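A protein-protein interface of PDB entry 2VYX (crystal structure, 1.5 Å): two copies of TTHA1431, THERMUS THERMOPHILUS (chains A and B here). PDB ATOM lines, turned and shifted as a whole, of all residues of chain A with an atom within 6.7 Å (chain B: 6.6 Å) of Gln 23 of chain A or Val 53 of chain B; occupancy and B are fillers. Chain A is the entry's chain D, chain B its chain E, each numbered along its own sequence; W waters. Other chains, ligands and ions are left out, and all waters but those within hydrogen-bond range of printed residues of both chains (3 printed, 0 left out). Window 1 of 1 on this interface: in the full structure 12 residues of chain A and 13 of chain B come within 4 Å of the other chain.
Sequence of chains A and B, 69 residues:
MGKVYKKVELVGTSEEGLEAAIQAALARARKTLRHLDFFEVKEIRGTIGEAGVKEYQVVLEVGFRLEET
OE1 of Gln 23 of chain A sits at hydrogen-bond distance from N of Val 53 of chain B (2.9 Å).
The backbone carbonyl oxygen (O) of Gly 46 of chain B is in hydrogen-bond range of the backbone NH (N) of Phe 39 of chain A.
NH2 of Arg 30 of chain A lies close to N of Gly 52 of chain B (3.1 Å).
Water W3 lies within hydrogen-bond range of OH of Tyr 56 of chain B and NE2 of Gln 23 of chain A.
Water W2 lies within hydrogen-bond range of the backbone carbonyl oxygen of Val 53 of chain B (2.6 Å), the side-chain amide nitrogen of Gln 23 of chain A (2.9 Å) and the backbone carbonyl oxygen of Ala 51 of chain B (2.9 Å).
Water W1 bridges NH2 of Arg 45 of chain B (2.8 Å) and O of Phe 39 of chain A (2.9 Å).
N of Tyr 56 of chain B sits at hydrogen-bond distance from O of Ser 14 of chain B, at 2.7 Å.
The backbone NH of Lys 54 of chain B lies within hydrogen-bond range of the backbone carbonyl oxygen of Thr 47 of chain B (2.9 Å).
The backbone NH (N) of Thr 47 of chain B sits at hydrogen-bond distance from the backbone carbonyl oxygen (O) of Glu 55 of chain B.
No position is printed for both chains.
CG of Glu 19 of chain A touches OH of Tyr 56 of chain B, 3.3 Å away.
Gln 23 of chain A touches Ala 51 of chain B (OE1 to O, 3.8 Å).
Gln 23 of chain A touches Gly 52 of chain B (OE1 to CA, 3.5 Å).
Leu 26 of chain A touches Ile 48 of chain B (CD2 to CD1, 3.5 Å).
C of Gly 52 of chain B touches CD1 of Leu 26 of chain A, 3.8 Å away.
Val 53 of chain B touches Leu 26 of chain A (N to CD1, 3.6 Å).
NH2 of Arg 30 of chain A touches C of Ala 51 of chain B (3.5 Å).
Arg 45 of chain B touches Phe 39 of chain A (CA to O, 3.3 Å).
Phe 39 of chain A touches Thr 47 of chain B (CE1 to O, 3.6 Å).
Phe 39 of chain A touches Ile 48 of chain B (CD1 to CG1, 3.97 Å).
Printed residues of chain B that touch a printed residue of chain A: Arg 45, Gly 46, Thr 47, Ile 48, Ala 51, Gly 52, Val 53 and Tyr 56.
Along chain B the printed residues that touch a printed residue of chain A span positions 45 to 56.
Of the 15 printed residues of chain A, 6 touch a printed residue of chain B.
Among the printed residues, 15 pairs touch across the chains.
Of the printed residues of chain B, Gln 23 of chain A touches Ala 51, Gly 52, Val 53 and Tyr 56.
Val 53 of chain B touches just these residues of chain A: Ile 22, Gln 23 and Leu 26.
Printed residues of chain A within 4 Å of Gly 46 of chain B: Phe 39 (2.9 Å).
Of the printed residues of chain B, Leu 26 of chain A touches Ile 48, Gly 52 and Val 53.
Printed residues of chain A within 4 Å of Ile 48 of chain B: Leu 26 (3.5 Å) and Phe 39 (3.97 Å).
Of the printed residues of chain A, Arg 45 of chain B touches Phe 39.
Lys 54 of chain B touches none of the printed residues of chain A.
The nearest residue of chain B that does not touch Gln 23 of chain A is Lys 54 of chain B (6.2 Å).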
ATOM      1  N   GLY A  12      14.347   5.827  27.646  1.00  0.00           N
ATOM      2  CA  GLY A  12      14.472   4.380  27.800  1.00  0.00           C
ATOM      3  C   GLY A  12      15.835   4.011  28.344  1.00  0.00           C
ATOM      4  O   GLY A  12      16.842   4.631  27.990  1.00  0.00           O
ATOM      5  N   LEU A  18      21.786  -0.188  23.128  1.00  0.00           N
ATOM      6  CA  LEU A  18      21.036   0.943  22.615  1.00  0.00           C
ATOM      7  C   LEU A  18      19.632   0.571  22.159  1.00  0.00           C
ATOM      8  O   LEU A  18      18.662   1.195  22.563  1.00  0.00           O
ATOM      9  CB  LEU A  18      21.805   1.599  21.458  1.00  0.00           C
ATOM     10  CG  LEU A  18      23.100   2.274  21.879  1.00  0.00           C
ATOM     11  CD1 LEU A  18      23.830   2.827  20.676  1.00  0.00           C
ATOM     12  CD2 LEU A  18      22.816   3.388  22.865  1.00  0.00           C
ATOM     13  N   GLU A  19      19.525  -0.435  21.295  1.00  0.00           N
ATOM     14  CA  GLU A  19      18.231  -0.863  20.798  1.00  0.00           C
ATOM     15  C   GLU A  19      17.332  -1.310  21.965  1.00  0.00           C
ATOM     16  O   GLU A  19      16.156  -0.986  21.999  1.00  0.00           O
ATOM     17  CB  GLU A  19      18.389  -1.983  19.764  1.00  0.00           C
ATOM     18  CG  GLU A  19      18.903  -1.511  18.398  1.00  0.00           C
ATOM     19  CD  GLU A  19      20.409  -1.571  18.258  1.00  0.00           C
ATOM     20  OE1 GLU A  19      21.117  -1.567  19.285  1.00  0.00           O
ATOM     21  OE2 GLU A  19      20.895  -1.631  17.107  1.00  0.00           O
ATOM     22  N   ALA A  20      17.911  -2.037  22.919  1.00  0.00           N
ATOM     23  CA  ALA A  20      17.175  -2.480  24.111  1.00  0.00           C
ATOM     24  C   ALA A  20      16.617  -1.304  24.917  1.00  0.00           C
ATOM     25  O   ALA A  20      15.493  -1.367  25.415  1.00  0.00           O
ATOM     26  CB  ALA A  20      18.066  -3.355  24.994  1.00  0.00           C
ATOM     27  N   ALA A  21      17.396  -0.229  25.033  1.00  0.00           N
ATOM     28  CA  ALA A  21      16.932   0.983  25.721  1.00  0.00           C
ATOM     29  C   ALA A  21      15.781   1.652  24.981  1.00  0.00           C
ATOM     30  O   ALA A  21      14.794   2.049  25.594  1.00  0.00           O
ATOM     31  CB  ALA A  21      18.082   1.967  25.914  1.00  0.00           C
ATOM     32  N   ILE A  22      15.892   1.753  23.661  1.00  0.00           N
ATOM     33  CA  ILE A  22      14.813   2.309  22.840  1.00  0.00           C
ATOM     34  C   ILE A  22      13.549   1.438  22.960  1.00  0.00           C
ATOM     35  O   ILE A  22      12.442   1.942  23.112  1.00  0.00           O
ATOM     36  CB  ILE A  22      15.226   2.435  21.348  1.00  0.00           C
ATOM     37  CG1 ILE A  22      16.279   3.552  21.156  1.00  0.00           C
ATOM     38  CG2 ILE A  22      14.024   2.710  20.479  1.00  0.00           C
ATOM     39  CD1 ILE A  22      16.960   3.516  19.800  1.00  0.00           C
ATOM     40  N   GLN A  23      13.726   0.125  22.901  1.00  0.00           N
ATOM     41  CA  GLN A  23      12.591  -0.799  22.967  1.00  0.00           C
ATOM     42  C   GLN A  23      11.892  -0.720  24.321  1.00  0.00           C
ATOM     43  O   GLN A  23      10.667  -0.853  24.391  1.00  0.00           O
ATOM     44  CB  GLN A  23      13.044  -2.234  22.688  1.00  0.00           C
ATOM     45  CG  GLN A  23      13.470  -2.495  21.247  1.00  0.00           C
ATOM     46  CD  GLN A  23      12.315  -2.744  20.306  1.00  0.00           C
ATOM     47  OE1 GLN A  23      11.232  -2.189  20.459  1.00  0.00           O
ATOM     48  NE2 GLN A  23      12.544  -3.587  19.315  1.00  0.00           N
ATOM     49  N   ALA A  24      12.659  -0.465  25.381  1.00  0.00           N
ATOM     50  CA  ALA A  24      12.100  -0.336  26.735  1.00  0.00           C
ATOM     51  C   ALA A  24      11.155   0.855  26.829  1.00  0.00           C
ATOM     52  O   ALA A  24      10.071   0.757  27.412  1.00  0.00           O
ATOM     53  CB  ALA A  24      13.205  -0.238  27.770  1.00  0.00           C
ATOM     54  N   ALA A  25      11.546   1.978  26.231  1.00  0.00           N
ATOM     55  CA  ALA A  25      10.692   3.158  26.212  1.00  0.00           C
ATOM     56  C   ALA A  25       9.415   2.906  25.430  1.00  0.00           C
ATOM     57  O   ALA A  25       8.340   3.277  25.873  1.00  0.00           O
ATOM     58  CB  ALA A  25      11.437   4.371  25.632  1.00  0.00           C
ATOM     59  N   LEU A  26       9.544   2.274  24.263  1.00  0.00           N
ATOM     60  CA  LEU A  26       8.410   2.000  23.405  1.00  0.00           C
ATOM     61  C   LEU A  26       7.469   0.948  23.997  1.00  0.00           C
ATOM     62  O   LEU A  26       6.251   1.066  23.863  1.00  0.00           O
ATOM     63  CB  LEU A  26       8.872   1.594  22.003  1.00  0.00           C
ATOM     64  CG  LEU A  26       9.573   2.660  21.148  1.00  0.00           C
ATOM     65  CD1 LEU A  26       9.790   2.115  19.739  1.00  0.00           C
ATOM     66  CD2 LEU A  26       8.790   3.963  21.102  1.00  0.00           C
ATOM     67  N   ALA A  27       8.037  -0.055  24.663  1.00  0.00           N
ATOM     68  CA  ALA A  27       7.239  -1.095  25.313  1.00  0.00           C
ATOM     69  C   ALA A  27       6.374  -0.487  26.398  1.00  0.00           C
ATOM     70  O   ALA A  27       5.222  -0.884  26.573  1.00  0.00           O
ATOM     71  CB  ALA A  27       8.137  -2.168  25.893  1.00  0.00           C
ATOM     72  N   ARG A  28       6.927   0.482  27.126  1.00  0.00           N
ATOM     73  CA  ARG A  28       6.167   1.218  28.130  1.00  0.00           C
ATOM     74  C   ARG A  28       5.086   2.116  27.519  1.00  0.00           C
ATOM     75  O   ARG A  28       3.959   2.159  28.009  1.00  0.00           O
ATOM     76  CB  ARG A  28       7.102   2.052  29.005  1.00  0.00           C
ATOM     77  CG  ARG A  28       6.410   2.886  30.062  1.00  0.00           C
ATOM     78  CD  ARG A  28       5.411   2.108  30.925  1.00  0.00           C
ATOM     79  NE  ARG A  28       4.686   3.020  31.813  1.00  0.00           N
ATOM     80  CZ  ARG A  28       3.589   3.703  31.484  1.00  0.00           C
ATOM     81  NH1 ARG A  28       3.043   3.632  30.274  1.00  0.00           N
ATOM     82  NH2 ARG A  28       3.039   4.489  32.381  1.00  0.00           N
ATOM     83  N   ARG A  30       3.512   1.685  24.784  1.00  0.00           N
ATOM     84  CA  ARG A  30       2.486   0.759  24.271  1.00  0.00           C
ATOM     85  C   ARG A  30       1.453   0.314  25.315  1.00  0.00           C
ATOM     86  O   ARG A  30       0.336  -0.081  24.966  1.00  0.00           O
ATOM     87  CB  ARG A  30       3.210  -0.475  23.709  1.00  0.00           C
ATOM     88  CG  ARG A  30       2.355  -1.607  23.170  1.00  0.00           C
ATOM     89  CD  ARG A  30       3.176  -2.566  22.273  1.00  0.00           C
ATOM     90  NE  ARG A  30       4.086  -3.476  22.984  1.00  0.00           N
ATOM     91  CZ  ARG A  30       5.424  -3.486  22.910  1.00  0.00           C
ATOM     92  NH1 ARG A  30       6.111  -4.383  23.613  1.00  0.00           N
ATOM     93  NH2 ARG A  30       6.097  -2.617  22.162  1.00  0.00           N
ATOM     94  N   PHE A  39       9.303   7.719  16.256  1.00  0.00           N
ATOM     95  CA  PHE A  39      10.207   8.152  17.315  1.00  0.00           C
ATOM     96  C   PHE A  39      11.432   8.870  16.750  1.00  0.00           C
ATOM     97  O   PHE A  39      11.796   8.702  15.594  1.00  0.00           O
ATOM     98  CB  PHE A  39      10.608   6.980  18.253  1.00  0.00           C
ATOM     99  CG  PHE A  39      11.501   5.939  17.622  1.00  0.00           C
ATOM    100  CD1 PHE A  39      10.962   4.816  17.006  1.00  0.00           C
ATOM    101  CD2 PHE A  39      12.883   6.074  17.666  1.00  0.00           C
ATOM    102  CE1 PHE A  39      11.787   3.870  16.434  1.00  0.00           C
ATOM    103  CE2 PHE A  39      13.723   5.107  17.107  1.00  0.00           C
ATOM    104  CZ  PHE A  39      13.168   4.011  16.492  1.00  0.00           C
ATOM    105  N   LEU A  60      14.324   9.874  23.883  1.00  0.00           N
ATOM    106  CA  LEU A  60      13.510   9.698  22.676  1.00  0.00           C
ATOM    107  C   LEU A  60      12.316  10.629  22.697  1.00  0.00           C
ATOM    108  O   LEU A  60      11.687  10.770  23.733  1.00  0.00           O
ATOM    109  CB  LEU A  60      12.859   8.288  22.663  1.00  0.00           C
ATOM    110  CG  LEU A  60      13.593   6.997  22.366  1.00  0.00           C
ATOM    111  CD1 LEU A  60      12.582   5.869  22.283  1.00  0.00           C
ATOM    112  CD2 LEU A  60      14.377   7.128  21.065  1.00  0.00           C
ATOM    113  N   SER B  14      16.223  -0.482   8.672  1.00  0.00           N
ATOM    114  CA  SER B  14      16.312  -1.878   9.067  1.00  0.00           C
ATOM    115  C   SER B  14      15.319  -2.164  10.175  1.00  0.00           C
ATOM    116  O   SER B  14      15.053  -1.316  11.028  1.00  0.00           O
ATOM    117  CB  SER B  14      17.714  -2.210   9.544  1.00  0.00           C
ATOM    118  OG  SER B  14      17.799  -3.577   9.929  1.00  0.00           O
ATOM    119  N   GLU B  15      14.774  -3.375  10.167  1.00  0.00           N
ATOM    120  CA  GLU B  15      13.980  -3.842  11.294  1.00  0.00           C
ATOM    121  C   GLU B  15      14.860  -4.506  12.349  1.00  0.00           C
ATOM    122  O   GLU B  15      14.376  -4.855  13.417  1.00  0.00           O
ATOM    123  CB  GLU B  15      12.901  -4.808  10.804  1.00  0.00           C
ATOM    124  CG  GLU B  15      12.082  -4.229   9.643  1.00  0.00           C
ATOM    125  CD  GLU B  15      10.751  -4.922   9.419  1.00  0.00           C
ATOM    126  OE1 GLU B  15      10.424  -5.873  10.166  1.00  0.00           O
ATOM    127  OE2 GLU B  15      10.026  -4.503   8.484  1.00  0.00           O
ATOM    128  N   ARG B  45      15.927   7.981  13.707  1.00  0.00           N
ATOM    129  CA  ARG B  45      14.476   8.051  13.765  1.00  0.00           C
ATOM    130  C   ARG B  45      13.941   6.635  13.560  1.00  0.00           C
ATOM    131  O   ARG B  45      14.699   5.673  13.410  1.00  0.00           O
ATOM    132  CB  ARG B  45      13.903   8.955  12.663  1.00  0.00           C
ATOM    133  CG  ARG B  45      14.536  10.314  12.513  1.00  0.00           C
ATOM    134  CD  ARG B  45      14.009  11.016  11.292  1.00  0.00           C
ATOM    135  NE  ARG B  45      12.608  11.383  11.429  1.00  0.00           N
ATOM    136  CZ  ARG B  45      12.157  12.415  12.144  1.00  0.00           C
ATOM    137  NH1 ARG B  45      12.991  13.218  12.791  1.00  0.00           N
ATOM    138  NH2 ARG B  45      10.855  12.649  12.211  1.00  0.00           N
ATOM    139  N   GLY B  46      12.626   6.512  13.551  1.00  0.00           N
ATOM    140  CA  GLY B  46      12.011   5.244  13.232  1.00  0.00           C
ATOM    141  C   GLY B  46      10.519   5.213  13.420  1.00  0.00           C
ATOM    142  O   GLY B  46       9.882   6.219  13.783  1.00  0.00           O
ATOM    143  N   THR B  47       9.965   4.039  13.147  1.00  0.00           N
ATOM    144  CA  THR B  47       8.528   3.837  13.195  1.00  0.00           C
ATOM    145  C   THR B  47       8.240   2.850  14.316  1.00  0.00           C
ATOM    146  O   THR B  47       9.114   2.098  14.746  1.00  0.00           O
ATOM    147  CB  THR B  47       7.954   3.304  11.859  1.00  0.00           C
ATOM    148  OG1 THR B  47       8.659   2.120  11.469  1.00  0.00           O
ATOM    149  CG2 THR B  47       8.036   4.366  10.758  1.00  0.00           C
ATOM    150  N   ILE B  48       7.008   2.898  14.796  1.00  0.00           N
ATOM    151  CA  ILE B  48       6.569   2.074  15.901  1.00  0.00           C
ATOM    152  C   ILE B  48       5.447   1.163  15.401  1.00  0.00           C
ATOM    153  O   ILE B  48       4.568   1.588  14.666  1.00  0.00           O
ATOM    154  CB  ILE B  48       6.058   2.939  17.070  1.00  0.00           C
ATOM    155  CG1 ILE B  48       7.100   4.007  17.436  1.00  0.00           C
ATOM    156  CG2 ILE B  48       5.713   2.057  18.274  1.00  0.00           C
ATOM    157  CD1 ILE B  48       6.656   4.975  18.474  1.00  0.00           C
ATOM    158  N   GLY B  49       5.496  -0.100  15.795  1.00  0.00           N
ATOM    159  CA  GLY B  49       4.435  -1.044  15.457  1.00  0.00           C
ATOM    160  C   GLY B  49       4.007  -1.839  16.671  1.00  0.00           C
ATOM    161  O   GLY B  49       4.285  -1.458  17.811  1.00  0.00           O
ATOM    162  N   ALA B  51       5.125  -4.527  17.954  1.00  0.00           N
ATOM    163  CA  ALA B  51       6.200  -5.082  18.779  1.00  0.00           C
ATOM    164  C   ALA B  51       7.254  -4.061  19.226  1.00  0.00           C
ATOM    165  O   ALA B  51       8.361  -4.445  19.590  1.00  0.00           O
ATOM    166  CB  ALA B  51       6.877  -6.216  18.036  1.00  0.00           C
ATOM    167  N   GLY B  52       6.908  -2.779  19.223  1.00  0.00           N
ATOM    168  CA  GLY B  52       7.859  -1.727  19.557  1.00  0.00           C
ATOM    169  C   GLY B  52       8.424  -1.106  18.298  1.00  0.00           C
ATOM    170  O   GLY B  52       7.673  -0.589  17.477  1.00  0.00           O
ATOM    171  N   VAL B  53       9.745  -1.143  18.147  1.00  0.00           N
ATOM    172  CA  VAL B  53      10.375  -0.606  16.943  1.00  0.00           C
ATOM    173  C   VAL B  53       9.931  -1.449  15.750  1.00  0.00           C
ATOM    174  O   VAL B  53      10.080  -2.668  15.755  1.00  0.00           O
ATOM    175  CB  VAL B  53      11.918  -0.647  16.995  1.00  0.00           C
ATOM    176  CG1 VAL B  53      12.500  -0.044  15.714  1.00  0.00           C
ATOM    177  CG2 VAL B  53      12.450   0.092  18.216  1.00  0.00           C
ATOM    178  N   LYS B  54       9.363  -0.797  14.749  1.00  0.00           N
ATOM    179  CA  LYS B  54       9.069  -1.452  13.487  1.00  0.00           C
ATOM    180  C   LYS B  54      10.309  -1.347  12.593  1.00  0.00           C
ATOM    181  O   LYS B  54      10.873  -2.356  12.145  1.00  0.00           O
ATOM    182  CB  LYS B  54       7.847  -0.803  12.831  1.00  0.00           C
ATOM    183  CG  LYS B  54       7.437  -1.448  11.519  1.00  0.00           C
ATOM    184  CD  LYS B  54       6.047  -1.024  11.099  1.00  0.00           C
ATOM    185  CE  LYS B  54       5.550  -1.880   9.935  1.00  0.00           C
ATOM    186  NZ  LYS B  54       4.172  -1.520   9.468  1.00  0.00           N
ATOM    187  N   GLU B  55      10.749  -0.113  12.367  1.00  0.00           N
ATOM    188  CA  GLU B  55      11.854   0.159  11.477  1.00  0.00           C
ATOM    189  C   GLU B  55      12.766   1.223  12.095  1.00  0.00           C
ATOM    190  O   GLU B  55      12.287   2.284  12.489  1.00  0.00           O
ATOM    191  CB  GLU B  55      11.268   0.642  10.162  1.00  0.00           C
ATOM    192  CG  GLU B  55      12.207   0.778   9.042  1.00  0.00           C
ATOM    193  CD  GLU B  55      11.479   1.123   7.768  1.00  0.00           C
ATOM    194  OE1 GLU B  55      11.391   2.322   7.429  1.00  0.00           O
ATOM    195  OE2 GLU B  55      10.954   0.195   7.120  1.00  0.00           O
ATOM    196  N   TYR B  56      14.057   0.920  12.209  1.00  0.00           N
ATOM    197  CA  TYR B  56      15.081   1.923  12.519  1.00  0.00           C
ATOM    198  C   TYR B  56      15.424   2.656  11.227  1.00  0.00           C
ATOM    199  O   TYR B  56      15.551   2.045  10.175  1.00  0.00           O
ATOM    200  CB  TYR B  56      16.343   1.268  13.067  1.00  0.00           C
ATOM    201  CG  TYR B  56      16.149   0.545  14.383  1.00  0.00           C
ATOM    202  CD1 TYR B  56      15.959  -0.830  14.413  1.00  0.00           C
ATOM    203  CD2 TYR B  56      16.166   1.236  15.595  1.00  0.00           C
ATOM    204  CE1 TYR B  56      15.789  -1.503  15.606  1.00  0.00           C
ATOM    205  CE2 TYR B  56      15.994   0.571  16.800  1.00  0.00           C
ATOM    206  CZ  TYR B  56      15.810  -0.805  16.798  1.00  0.00           C
ATOM    207  OH  TYR B  56      15.620  -1.497  17.981  1.00  0.00           O
HETATM  208  O   HOH W   1      10.469  10.355  13.688  1.00  0.00           O
HETATM  209  O   HOH W   2      10.477  -4.536  17.540  1.00  0.00           O
HETATM  210  O   HOH W   3      15.330  -3.900  17.967  1.00  0.00           O
